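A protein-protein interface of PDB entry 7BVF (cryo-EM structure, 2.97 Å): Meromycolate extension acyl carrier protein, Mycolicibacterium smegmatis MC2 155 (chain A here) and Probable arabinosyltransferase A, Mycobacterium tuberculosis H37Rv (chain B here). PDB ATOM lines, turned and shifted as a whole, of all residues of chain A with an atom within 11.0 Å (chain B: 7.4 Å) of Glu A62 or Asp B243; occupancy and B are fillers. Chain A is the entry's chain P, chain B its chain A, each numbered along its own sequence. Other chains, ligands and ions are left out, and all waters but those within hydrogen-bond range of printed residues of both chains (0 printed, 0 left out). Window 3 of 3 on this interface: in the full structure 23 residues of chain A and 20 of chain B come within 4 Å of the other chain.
Of the printed residues of chain B, Glu A52 touches Arg B237 (3.0 Å).
Of the printed residues of chain B, Ile A59 touches Arg B237 (3.3 Å).
Printed residues of chain B within 4 Å of Asp A61: Arg B237 (3.4 Å), Arg B239 (3.4 Å) and Tyr B248 (3.7 Å).
Glu A62 touches three residues of chain B.
Asp A63 touches none of the printed residues of chain B.
Printed residues of chain B within 4 Å of Leu A64: Arg B237.
Gly B238 touches two residues of chain A.
Of chain A, only Asp A61 and Glu A62 come within 4 Å of Arg B239.
No residue of chain A comes within 4 Å of Thr B240.
Printed residues of chain A within 4 Å of Asp B243: Glu A62 (3.97 Å).
Leu B245 touches none of the printed residues of chain A.
Printed residues of chain A within 4 Å of Tyr B248: Asp A61 and Glu A62.
OE1 of Glu A52 lies within salt-bridge range of NH2 of Arg B237, 3.0 Å away.
OH of Tyr B248 sits close to OE2 of Glu A62, at 3.4 Å.
The guanidinium group (NH2) of Arg B239 is in salt-bridge range of the side-chain carboxylate (OD1) of Asp A61 (3.4 Å).
NH2 of Arg B237 sits at hydrogen-bond distance from O of Ile A59 (3.3 Å).
The backbone carbonyl oxygen of Arg B237 sits at hydrogen-bond distance from the backbone NH of Asp A61, at 3.4 Å.
Of the 13 printed residues of chain B, 5 touch a printed residue of chain A.
Among the printed residues, 11 pairs touch across the chains.
Among the printed residues, pairs that only touch across the chains: Lys A58 with Gly B238 (3.97 Å), Pro A60 with Gly B238 (3.9 Å), Asp A61 with Tyr B248 (3.7 Å), Glu A62 with Arg B239 (3.8 Å), Glu A62 with Asp B243 (3.97 Å) and Leu A64 with Arg B237 (3.6 Å).
The side-chain carboxylate (OE2) of Glu A52 lies within salt-bridge range of the side-chain amino group (NZ) of Lys A58 (3.5 Å).
NH1 of Arg B239 is in hydrogen-bond range of O of Asp B243, 2.8 Å away.
The side-chain carboxylate (OE1) of Glu A52 sits at hydrogen-bond distance from the backbone NH (N) of Ile A59 (3.5 Å).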
ATOM      1  N   SER A  41     -17.712 -26.768  28.990  1.00  0.00           N
ATOM      2  CA  SER A  41     -17.611 -25.343  29.285  1.00  0.00           C
ATOM      3  C   SER A  41     -16.167 -24.927  29.539  1.00  0.00           C
ATOM      4  O   SER A  41     -15.735 -23.862  29.084  1.00  0.00           O
ATOM      5  CB  SER A  41     -18.495 -24.999  30.484  1.00  0.00           C
ATOM      6  OG  SER A  41     -18.426 -23.621  30.799  1.00  0.00           O
ATOM      7  N   MET A  44     -14.345 -24.785  26.198  1.00  0.00           N
ATOM      8  CA  MET A  44     -14.833 -23.661  25.406  1.00  0.00           C
ATOM      9  C   MET A  44     -14.239 -22.345  25.898  1.00  0.00           C
ATOM     10  O   MET A  44     -13.770 -21.524  25.101  1.00  0.00           O
ATOM     11  CB  MET A  44     -16.359 -23.611  25.446  1.00  0.00           C
ATOM     12  CG  MET A  44     -17.035 -24.204  24.224  1.00  0.00           C
ATOM     13  SD  MET A  44     -16.282 -23.685  22.672  1.00  0.00           S
ATOM     14  CE  MET A  44     -16.557 -21.916  22.721  1.00  0.00           C
ATOM     15  N   VAL A  45     -14.241 -22.132  27.216  1.00  0.00           N
ATOM     16  CA  VAL A  45     -13.677 -20.894  27.742  1.00  0.00           C
ATOM     17  C   VAL A  45     -12.169 -20.852  27.551  1.00  0.00           C
ATOM     18  O   VAL A  45     -11.604 -19.783  27.306  1.00  0.00           O
ATOM     19  CB  VAL A  45     -14.062 -20.696  29.218  1.00  0.00           C
ATOM     20  CG1 VAL A  45     -13.633 -19.326  29.685  1.00  0.00           C
ATOM     21  CG2 VAL A  45     -15.556 -20.826  29.384  1.00  0.00           C
ATOM     22  N   ALA A  48     -11.675 -19.744  23.990  1.00  0.00           N
ATOM     23  CA  ALA A  48     -11.981 -18.327  23.841  1.00  0.00           C
ATOM     24  C   ALA A  48     -10.960 -17.434  24.530  1.00  0.00           C
ATOM     25  O   ALA A  48     -10.822 -16.267  24.153  1.00  0.00           O
ATOM     26  CB  ALA A  48     -13.376 -18.027  24.383  1.00  0.00           C
ATOM     27  N   GLU A  52      -7.725 -14.979  22.313  1.00  0.00           N
ATOM     28  CA  GLU A  52      -7.594 -13.550  22.551  1.00  0.00           C
ATOM     29  C   GLU A  52      -6.146 -13.106  22.659  1.00  0.00           C
ATOM     30  O   GLU A  52      -5.874 -11.904  22.591  1.00  0.00           O
ATOM     31  CB  GLU A  52      -8.330 -13.154  23.832  1.00  0.00           C
ATOM     32  CG  GLU A  52      -9.833 -13.059  23.684  1.00  0.00           C
ATOM     33  CD  GLU A  52     -10.547 -12.982  25.018  1.00  0.00           C
ATOM     34  OE1 GLU A  52     -11.623 -13.599  25.156  1.00  0.00           O
ATOM     35  OE2 GLU A  52     -10.031 -12.304  25.932  1.00  0.00           O
ATOM     36  N   LYS A  58     -11.983  -9.320  21.833  1.00  0.00           N
ATOM     37  CA  LYS A  58     -12.699  -9.674  23.053  1.00  0.00           C
ATOM     38  C   LYS A  58     -13.887 -10.567  22.717  1.00  0.00           C
ATOM     39  O   LYS A  58     -14.831 -10.135  22.050  1.00  0.00           O
ATOM     40  CB  LYS A  58     -13.154  -8.414  23.780  1.00  0.00           C
ATOM     41  CG  LYS A  58     -13.831  -8.687  25.112  1.00  0.00           C
ATOM     42  CD  LYS A  58     -12.839  -8.625  26.259  1.00  0.00           C
ATOM     43  CE  LYS A  58     -13.343  -9.401  27.461  1.00  0.00           C
ATOM     44  NZ  LYS A  58     -12.810 -10.789  27.483  1.00  0.00           N
ATOM     45  N   ILE A  59     -13.842 -11.814  23.176  1.00  0.00           N
ATOM     46  CA  ILE A  59     -14.993 -12.707  23.101  1.00  0.00           C
ATOM     47  C   ILE A  59     -15.569 -12.839  24.505  1.00  0.00           C
ATOM     48  O   ILE A  59     -15.047 -13.621  25.314  1.00  0.00           O
ATOM     49  CB  ILE A  59     -14.616 -14.079  22.527  1.00  0.00           C
ATOM     50  CG1 ILE A  59     -13.792 -13.922  21.251  1.00  0.00           C
ATOM     51  CG2 ILE A  59     -15.862 -14.888  22.239  1.00  0.00           C
ATOM     52  CD1 ILE A  59     -13.515 -15.225  20.544  1.00  0.00           C
ATOM     53  N   PRO A  60     -16.620 -12.100  24.846  1.00  0.00           N
ATOM     54  CA  PRO A  60     -17.194 -12.203  26.191  1.00  0.00           C
ATOM     55  C   PRO A  60     -17.864 -13.550  26.401  1.00  0.00           C
ATOM     56  O   PRO A  60     -18.110 -14.316  25.468  1.00  0.00           O
ATOM     57  CB  PRO A  60     -18.208 -11.059  26.234  1.00  0.00           C
ATOM     58  CG  PRO A  60     -18.564 -10.826  24.815  1.00  0.00           C
ATOM     59  CD  PRO A  60     -17.327 -11.110  24.019  1.00  0.00           C
ATOM     60  N   ASP A  61     -18.163 -13.836  27.667  1.00  0.00           N
ATOM     61  CA  ASP A  61     -18.765 -15.115  28.015  1.00  0.00           C
ATOM     62  C   ASP A  61     -20.234 -15.190  27.621  1.00  0.00           C
ATOM     63  O   ASP A  61     -20.753 -16.292  27.414  1.00  0.00           O
ATOM     64  CB  ASP A  61     -18.601 -15.375  29.513  1.00  0.00           C
ATOM     65  CG  ASP A  61     -18.534 -16.852  29.850  1.00  0.00           C
ATOM     66  OD1 ASP A  61     -17.820 -17.207  30.810  1.00  0.00           O
ATOM     67  OD2 ASP A  61     -19.190 -17.659  29.162  1.00  0.00           O
ATOM     68  N   GLU A  62     -20.910 -14.049  27.495  1.00  0.00           N
ATOM     69  CA  GLU A  62     -22.280 -14.005  27.000  1.00  0.00           C
ATOM     70  C   GLU A  62     -22.355 -14.041  25.482  1.00  0.00           C
ATOM     71  O   GLU A  62     -23.402 -13.717  24.911  1.00  0.00           O
ATOM     72  CB  GLU A  62     -22.991 -12.755  27.524  1.00  0.00           C
ATOM     73  CG  GLU A  62     -23.519 -12.881  28.943  1.00  0.00           C
ATOM     74  CD  GLU A  62     -22.502 -12.461  29.988  1.00  0.00           C
ATOM     75  OE1 GLU A  62     -21.289 -12.637  29.748  1.00  0.00           O
ATOM     76  OE2 GLU A  62     -22.917 -11.952  31.050  1.00  0.00           O
ATOM     77  N   ASP A  63     -21.268 -14.422  24.825  1.00  0.00           N
ATOM     78  CA  ASP A  63     -21.161 -14.443  23.374  1.00  0.00           C
ATOM     79  C   ASP A  63     -20.874 -15.829  22.823  1.00  0.00           C
ATOM     80  O   ASP A  63     -21.467 -16.222  21.817  1.00  0.00           O
ATOM     81  CB  ASP A  63     -20.058 -13.472  22.930  1.00  0.00           C
ATOM     82  CG  ASP A  63     -19.978 -13.313  21.429  1.00  0.00           C
ATOM     83  OD1 ASP A  63     -20.887 -13.783  20.716  1.00  0.00           O
ATOM     84  OD2 ASP A  63     -18.991 -12.711  20.961  1.00  0.00           O
ATOM     85  N   LEU A  64     -19.988 -16.590  23.466  1.00  0.00           N
ATOM     86  CA  LEU A  64     -19.680 -17.939  23.009  1.00  0.00           C
ATOM     87  C   LEU A  64     -20.809 -18.927  23.272  1.00  0.00           C
ATOM     88  O   LEU A  64     -20.645 -20.116  22.981  1.00  0.00           O
ATOM     89  CB  LEU A  64     -18.383 -18.431  23.659  1.00  0.00           C
ATOM     90  CG  LEU A  64     -18.286 -18.519  25.185  1.00  0.00           C
ATOM     91  CD1 LEU A  64     -18.720 -19.881  25.707  1.00  0.00           C
ATOM     92  CD2 LEU A  64     -16.872 -18.201  25.635  1.00  0.00           C
ATOM     93  N   ALA A  65     -21.940 -18.476  23.816  1.00  0.00           N
ATOM     94  CA  ALA A  65     -23.105 -19.340  23.942  1.00  0.00           C
ATOM     95  C   ALA A  65     -23.811 -19.558  22.612  1.00  0.00           C
ATOM     96  O   ALA A  65     -24.524 -20.556  22.457  1.00  0.00           O
ATOM     97  CB  ALA A  65     -24.088 -18.758  24.959  1.00  0.00           C
ATOM     98  N   GLY A  66     -23.631 -18.653  21.653  1.00  0.00           N
ATOM     99  CA  GLY A  66     -24.227 -18.762  20.341  1.00  0.00           C
ATOM    100  C   GLY A  66     -23.292 -19.227  19.246  1.00  0.00           C
ATOM    101  O   GLY A  66     -23.677 -19.194  18.071  1.00  0.00           O
ATOM    102  N   LEU A  67     -22.075 -19.652  19.586  1.00  0.00           N
ATOM    103  CA  LEU A  67     -21.140 -20.212  18.611  1.00  0.00           C
ATOM    104  C   LEU A  67     -21.259 -21.731  18.684  1.00  0.00           C
ATOM    105  O   LEU A  67     -20.509 -22.414  19.380  1.00  0.00           O
ATOM    106  CB  LEU A  67     -19.719 -19.731  18.885  1.00  0.00           C
ATOM    107  CG  LEU A  67     -19.544 -18.231  19.131  1.00  0.00           C
ATOM    108  CD1 LEU A  67     -18.072 -17.875  19.269  1.00  0.00           C
ATOM    109  CD2 LEU A  67     -20.190 -17.419  18.022  1.00  0.00           C
ATOM    110  N   ARG A  68     -22.232 -22.262  17.945  1.00  0.00           N
ATOM    111  CA  ARG A  68     -22.558 -23.681  18.048  1.00  0.00           C
ATOM    112  C   ARG A  68     -21.580 -24.539  17.258  1.00  0.00           C
ATOM    113  O   ARG A  68     -21.080 -25.549  17.766  1.00  0.00           O
ATOM    114  CB  ARG A  68     -23.989 -23.922  17.571  1.00  0.00           C
ATOM    115  CG  ARG A  68     -24.657 -25.131  18.200  1.00  0.00           C
ATOM    116  CD  ARG A  68     -26.173 -25.000  18.173  1.00  0.00           C
ATOM    117  NE  ARG A  68     -26.617 -23.608  18.249  1.00  0.00           N
ATOM    118  CZ  ARG A  68     -26.584 -22.862  19.350  1.00  0.00           C
ATOM    119  NH1 ARG A  68     -26.126 -23.366  20.488  1.00  0.00           N
ATOM    120  NH2 ARG A  68     -27.009 -21.608  19.312  1.00  0.00           N
ATOM    121  N   TYR A  76     -18.836 -15.352  12.993  1.00  0.00           N
ATOM    122  CA  TYR A  76     -18.766 -14.306  14.007  1.00  0.00           C
ATOM    123  C   TYR A  76     -17.528 -13.440  13.822  1.00  0.00           C
ATOM    124  O   TYR A  76     -17.622 -12.210  13.725  1.00  0.00           O
ATOM    125  CB  TYR A  76     -18.783 -14.931  15.403  1.00  0.00           C
ATOM    126  CG  TYR A  76     -18.293 -14.001  16.488  1.00  0.00           C
ATOM    127  CD1 TYR A  76     -19.114 -13.005  16.994  1.00  0.00           C
ATOM    128  CD2 TYR A  76     -17.011 -14.122  17.006  1.00  0.00           C
ATOM    129  CE1 TYR A  76     -18.673 -12.154  17.980  1.00  0.00           C
ATOM    130  CE2 TYR A  76     -16.560 -13.273  17.993  1.00  0.00           C
ATOM    131  CZ  TYR A  76     -17.396 -12.290  18.476  1.00  0.00           C
ATOM    132  OH  TYR A  76     -16.957 -11.440  19.464  1.00  0.00           O
ATOM    133  N   ARG B 234     -14.576 -11.414  37.377  1.00  0.00           N
ATOM    134  CA  ARG B 234     -15.845 -11.436  36.653  1.00  0.00           C
ATOM    135  C   ARG B 234     -15.959 -10.266  35.689  1.00  0.00           C
ATOM    136  O   ARG B 234     -16.558 -10.403  34.619  1.00  0.00           O
ATOM    137  CB  ARG B 234     -17.023 -11.419  37.625  1.00  0.00           C
ATOM    138  CG  ARG B 234     -17.003 -12.522  38.659  1.00  0.00           C
ATOM    139  CD  ARG B 234     -17.030 -13.897  38.029  1.00  0.00           C
ATOM    140  NE  ARG B 234     -17.148 -14.940  39.041  1.00  0.00           N
ATOM    141  CZ  ARG B 234     -16.115 -15.503  39.655  1.00  0.00           C
ATOM    142  NH1 ARG B 234     -14.881 -15.125  39.360  1.00  0.00           N
ATOM    143  NH2 ARG B 234     -16.312 -16.444  40.566  1.00  0.00           N
ATOM    144  N   ARG B 237     -14.125 -10.626  32.008  1.00  0.00           N
ATOM    145  CA  ARG B 237     -14.639 -11.566  31.017  1.00  0.00           C
ATOM    146  C   ARG B 237     -15.972 -11.115  30.446  1.00  0.00           C
ATOM    147  O   ARG B 237     -16.859 -11.931  30.192  1.00  0.00           O
ATOM    148  CB  ARG B 237     -14.758 -12.960  31.621  1.00  0.00           C
ATOM    149  CG  ARG B 237     -13.457 -13.740  31.632  1.00  0.00           C
ATOM    150  CD  ARG B 237     -13.021 -14.102  30.223  1.00  0.00           C
ATOM    151  NE  ARG B 237     -14.010 -14.932  29.542  1.00  0.00           N
ATOM    152  CZ  ARG B 237     -13.954 -15.256  28.255  1.00  0.00           C
ATOM    153  NH1 ARG B 237     -14.898 -16.015  27.719  1.00  0.00           N
ATOM    154  NH2 ARG B 237     -12.954 -14.817  27.504  1.00  0.00           N
ATOM    155  N   GLY B 238     -16.145  -9.809  30.249  1.00  0.00           N
ATOM    156  CA  GLY B 238     -17.342  -9.277  29.641  1.00  0.00           C
ATOM    157  C   GLY B 238     -18.602  -9.374  30.468  1.00  0.00           C
ATOM    158  O   GLY B 238     -19.638  -8.852  30.040  1.00  0.00           O
ATOM    159  N   ARG B 239     -18.559 -10.015  31.633  1.00  0.00           N
ATOM    160  CA  ARG B 239     -19.738 -10.120  32.476  1.00  0.00           C
ATOM    161  C   ARG B 239     -20.066  -8.762  33.091  1.00  0.00           C
ATOM    162  O   ARG B 239     -19.344  -7.777  32.921  1.00  0.00           O
ATOM    163  CB  ARG B 239     -19.524 -11.172  33.561  1.00  0.00           C
ATOM    164  CG  ARG B 239     -19.481 -12.596  33.045  1.00  0.00           C
ATOM    165  CD  ARG B 239     -19.191 -13.571  34.169  1.00  0.00           C
ATOM    166  NE  ARG B 239     -19.225 -14.957  33.716  1.00  0.00           N
ATOM    167  CZ  ARG B 239     -20.333 -15.683  33.633  1.00  0.00           C
ATOM    168  NH1 ARG B 239     -21.498 -15.152  33.972  1.00  0.00           N
ATOM    169  NH2 ARG B 239     -20.278 -16.938  33.212  1.00  0.00           N
ATOM    170  N   THR B 240     -21.182  -8.712  33.820  1.00  0.00           N
ATOM    171  CA  THR B 240     -21.644  -7.484  34.459  1.00  0.00           C
ATOM    172  C   THR B 240     -21.785  -7.643  35.968  1.00  0.00           C
ATOM    173  O   THR B 240     -22.523  -6.880  36.596  1.00  0.00           O
ATOM    174  CB  THR B 240     -22.976  -7.029  33.861  1.00  0.00           C
ATOM    175  OG1 THR B 240     -24.045  -7.779  34.450  1.00  0.00           O
ATOM    176  CG2 THR B 240     -22.992  -7.232  32.352  1.00  0.00           C
ATOM    177  N   LEU B 241     -21.097  -8.628  36.554  1.00  0.00           N
ATOM    178  CA  LEU B 241     -21.164  -8.958  37.978  1.00  0.00           C
ATOM    179  C   LEU B 241     -22.594  -8.968  38.514  1.00  0.00           C
ATOM    180  O   LEU B 241     -22.834  -8.655  39.684  1.00  0.00           O
ATOM    181  CB  LEU B 241     -20.269  -8.017  38.800  1.00  0.00           C
ATOM    182  CG  LEU B 241     -20.331  -6.487  38.756  1.00  0.00           C
ATOM    183  CD1 LEU B 241     -21.434  -5.908  39.629  1.00  0.00           C
ATOM    184  CD2 LEU B 241     -18.983  -5.931  39.172  1.00  0.00           C
ATOM    185  N   ARG B 242     -23.542  -9.349  37.664  1.00  0.00           N
ATOM    186  CA  ARG B 242     -24.910  -9.628  38.071  1.00  0.00           C
ATOM    187  C   ARG B 242     -25.368 -11.022  37.680  1.00  0.00           C
ATOM    188  O   ARG B 242     -26.236 -11.583  38.349  1.00  0.00           O
ATOM    189  CB  ARG B 242     -25.873  -8.595  37.468  1.00  0.00           C
ATOM    190  CG  ARG B 242     -25.797  -7.234  38.135  1.00  0.00           C
ATOM    191  CD  ARG B 242     -26.694  -6.222  37.450  1.00  0.00           C
ATOM    192  NE  ARG B 242     -26.864  -5.017  38.256  1.00  0.00           N
ATOM    193  CZ  ARG B 242     -25.979  -4.028  38.318  1.00  0.00           C
ATOM    194  NH1 ARG B 242     -26.218  -2.969  39.080  1.00  0.00           N
ATOM    195  NH2 ARG B 242     -24.854  -4.095  37.620  1.00  0.00           N
ATOM    196  N   ASP B 243     -24.805 -11.590  36.615  1.00  0.00           N
ATOM    197  CA  ASP B 243     -24.997 -13.000  36.285  1.00  0.00           C
ATOM    198  C   ASP B 243     -23.843 -13.826  36.855  1.00  0.00           C
ATOM    199  O   ASP B 243     -23.111 -14.514  36.146  1.00  0.00           O
ATOM    200  CB  ASP B 243     -25.115 -13.176  34.776  1.00  0.00           C
ATOM    201  CG  ASP B 243     -26.369 -12.542  34.211  1.00  0.00           C
ATOM    202  OD1 ASP B 243     -27.373 -12.446  34.948  1.00  0.00           O
ATOM    203  OD2 ASP B 243     -26.353 -12.141  33.029  1.00  0.00           O
ATOM    204  N   TRP B 244     -23.690 -13.734  38.173  1.00  0.00           N
ATOM    205  CA  TRP B 244     -22.577 -14.360  38.886  1.00  0.00           C
ATOM    206  C   TRP B 244     -22.732 -15.876  38.829  1.00  0.00           C
ATOM    207  O   TRP B 244     -23.562 -16.457  39.531  1.00  0.00           O
ATOM    208  CB  TRP B 244     -22.538 -13.851  40.325  1.00  0.00           C
ATOM    209  CG  TRP B 244     -21.204 -13.984  41.006  1.00  0.00           C
ATOM    210  CD1 TRP B 244     -20.505 -15.132  41.219  1.00  0.00           C
ATOM    211  CD2 TRP B 244     -20.415 -12.926  41.572  1.00  0.00           C
ATOM    212  NE1 TRP B 244     -19.329 -14.860  41.875  1.00  0.00           N
ATOM    213  CE2 TRP B 244     -19.251 -13.512  42.104  1.00  0.00           C
ATOM    214  CE3 TRP B 244     -20.581 -11.541  41.678  1.00  0.00           C
ATOM    215  CZ2 TRP B 244     -18.260 -12.765  42.731  1.00  0.00           C
ATOM    216  CZ3 TRP B 244     -19.594 -10.803  42.302  1.00  0.00           C
ATOM    217  CH2 TRP B 244     -18.450 -11.416  42.819  1.00  0.00           C
ATOM    218  N   LEU B 245     -21.925 -16.521  37.982  1.00  0.00           N
ATOM    219  CA  LEU B 245     -21.906 -17.977  37.810  1.00  0.00           C
ATOM    220  C   LEU B 245     -23.288 -18.514  37.423  1.00  0.00           C
ATOM    221  O   LEU B 245     -23.935 -19.263  38.156  1.00  0.00           O
ATOM    222  CB  LEU B 245     -21.365 -18.682  39.061  1.00  0.00           C
ATOM    223  CG  LEU B 245     -19.847 -18.879  39.111  1.00  0.00           C
ATOM    224  CD1 LEU B 245     -19.115 -17.567  39.304  1.00  0.00           C
ATOM    225  CD2 LEU B 245     -19.465 -19.880  40.198  1.00  0.00           C
ATOM    226  N   THR B 246     -23.721 -18.100  36.235  1.00  0.00           N
ATOM    227  CA  THR B 246     -24.891 -18.666  35.572  1.00  0.00           C
ATOM    228  C   THR B 246     -24.395 -19.446  34.360  1.00  0.00           C
ATOM    229  O   THR B 246     -23.928 -18.852  33.382  1.00  0.00           O
ATOM    230  CB  THR B 246     -25.881 -17.579  35.162  1.00  0.00           C
ATOM    231  OG1 THR B 246     -25.431 -16.952  33.954  1.00  0.00           O
ATOM    232  CG2 THR B 246     -26.002 -16.532  36.255  1.00  0.00           C
ATOM    233  N   ARG B 247     -24.491 -20.772  34.429  1.00  0.00           N
ATOM    234  CA  ARG B 247     -23.949 -21.624  33.380  1.00  0.00           C
ATOM    235  C   ARG B 247     -24.684 -21.408  32.061  1.00  0.00           C
ATOM    236  O   ARG B 247     -25.863 -21.047  32.029  1.00  0.00           O
ATOM    237  CB  ARG B 247     -24.036 -23.096  33.782  1.00  0.00           C
ATOM    238  CG  ARG B 247     -23.054 -23.516  34.863  1.00  0.00           C
ATOM    239  CD  ARG B 247     -22.834 -25.021  34.842  1.00  0.00           C
ATOM    240  NE  ARG B 247     -22.154 -25.496  36.043  1.00  0.00           N
ATOM    241  CZ  ARG B 247     -22.759 -26.115  37.051  1.00  0.00           C
ATOM    242  NH1 ARG B 247     -24.066 -26.339  37.005  1.00  0.00           N
ATOM    243  NH2 ARG B 247     -22.060 -26.512  38.104  1.00  0.00           N
ATOM    244  N   TYR B 248     -23.966 -21.639  30.964  1.00  0.00           N
ATOM    245  CA  TYR B 248     -24.516 -21.520  29.622  1.00  0.00           C
ATOM    246  C   TYR B 248     -24.548 -22.832  28.858  1.00  0.00           C
ATOM    247  O   TYR B 248     -25.560 -23.131  28.221  1.00  0.00           O
ATOM    248  CB  TYR B 248     -23.714 -20.496  28.803  1.00  0.00           C
ATOM    249  CG  TYR B 248     -23.675 -19.115  29.413  1.00  0.00           C
ATOM    250  CD1 TYR B 248     -24.749 -18.246  29.279  1.00  0.00           C
ATOM    251  CD2 TYR B 248     -22.565 -18.678  30.118  1.00  0.00           C
ATOM    252  CE1 TYR B 248     -24.719 -16.982  29.834  1.00  0.00           C
ATOM    253  CE2 TYR B 248     -22.525 -17.416  30.676  1.00  0.00           C
ATOM    254  CZ  TYR B 248     -23.604 -16.572  30.531  1.00  0.00           C
ATOM    255  OH  TYR B 248     -23.568 -15.315  31.085  1.00  0.00           O
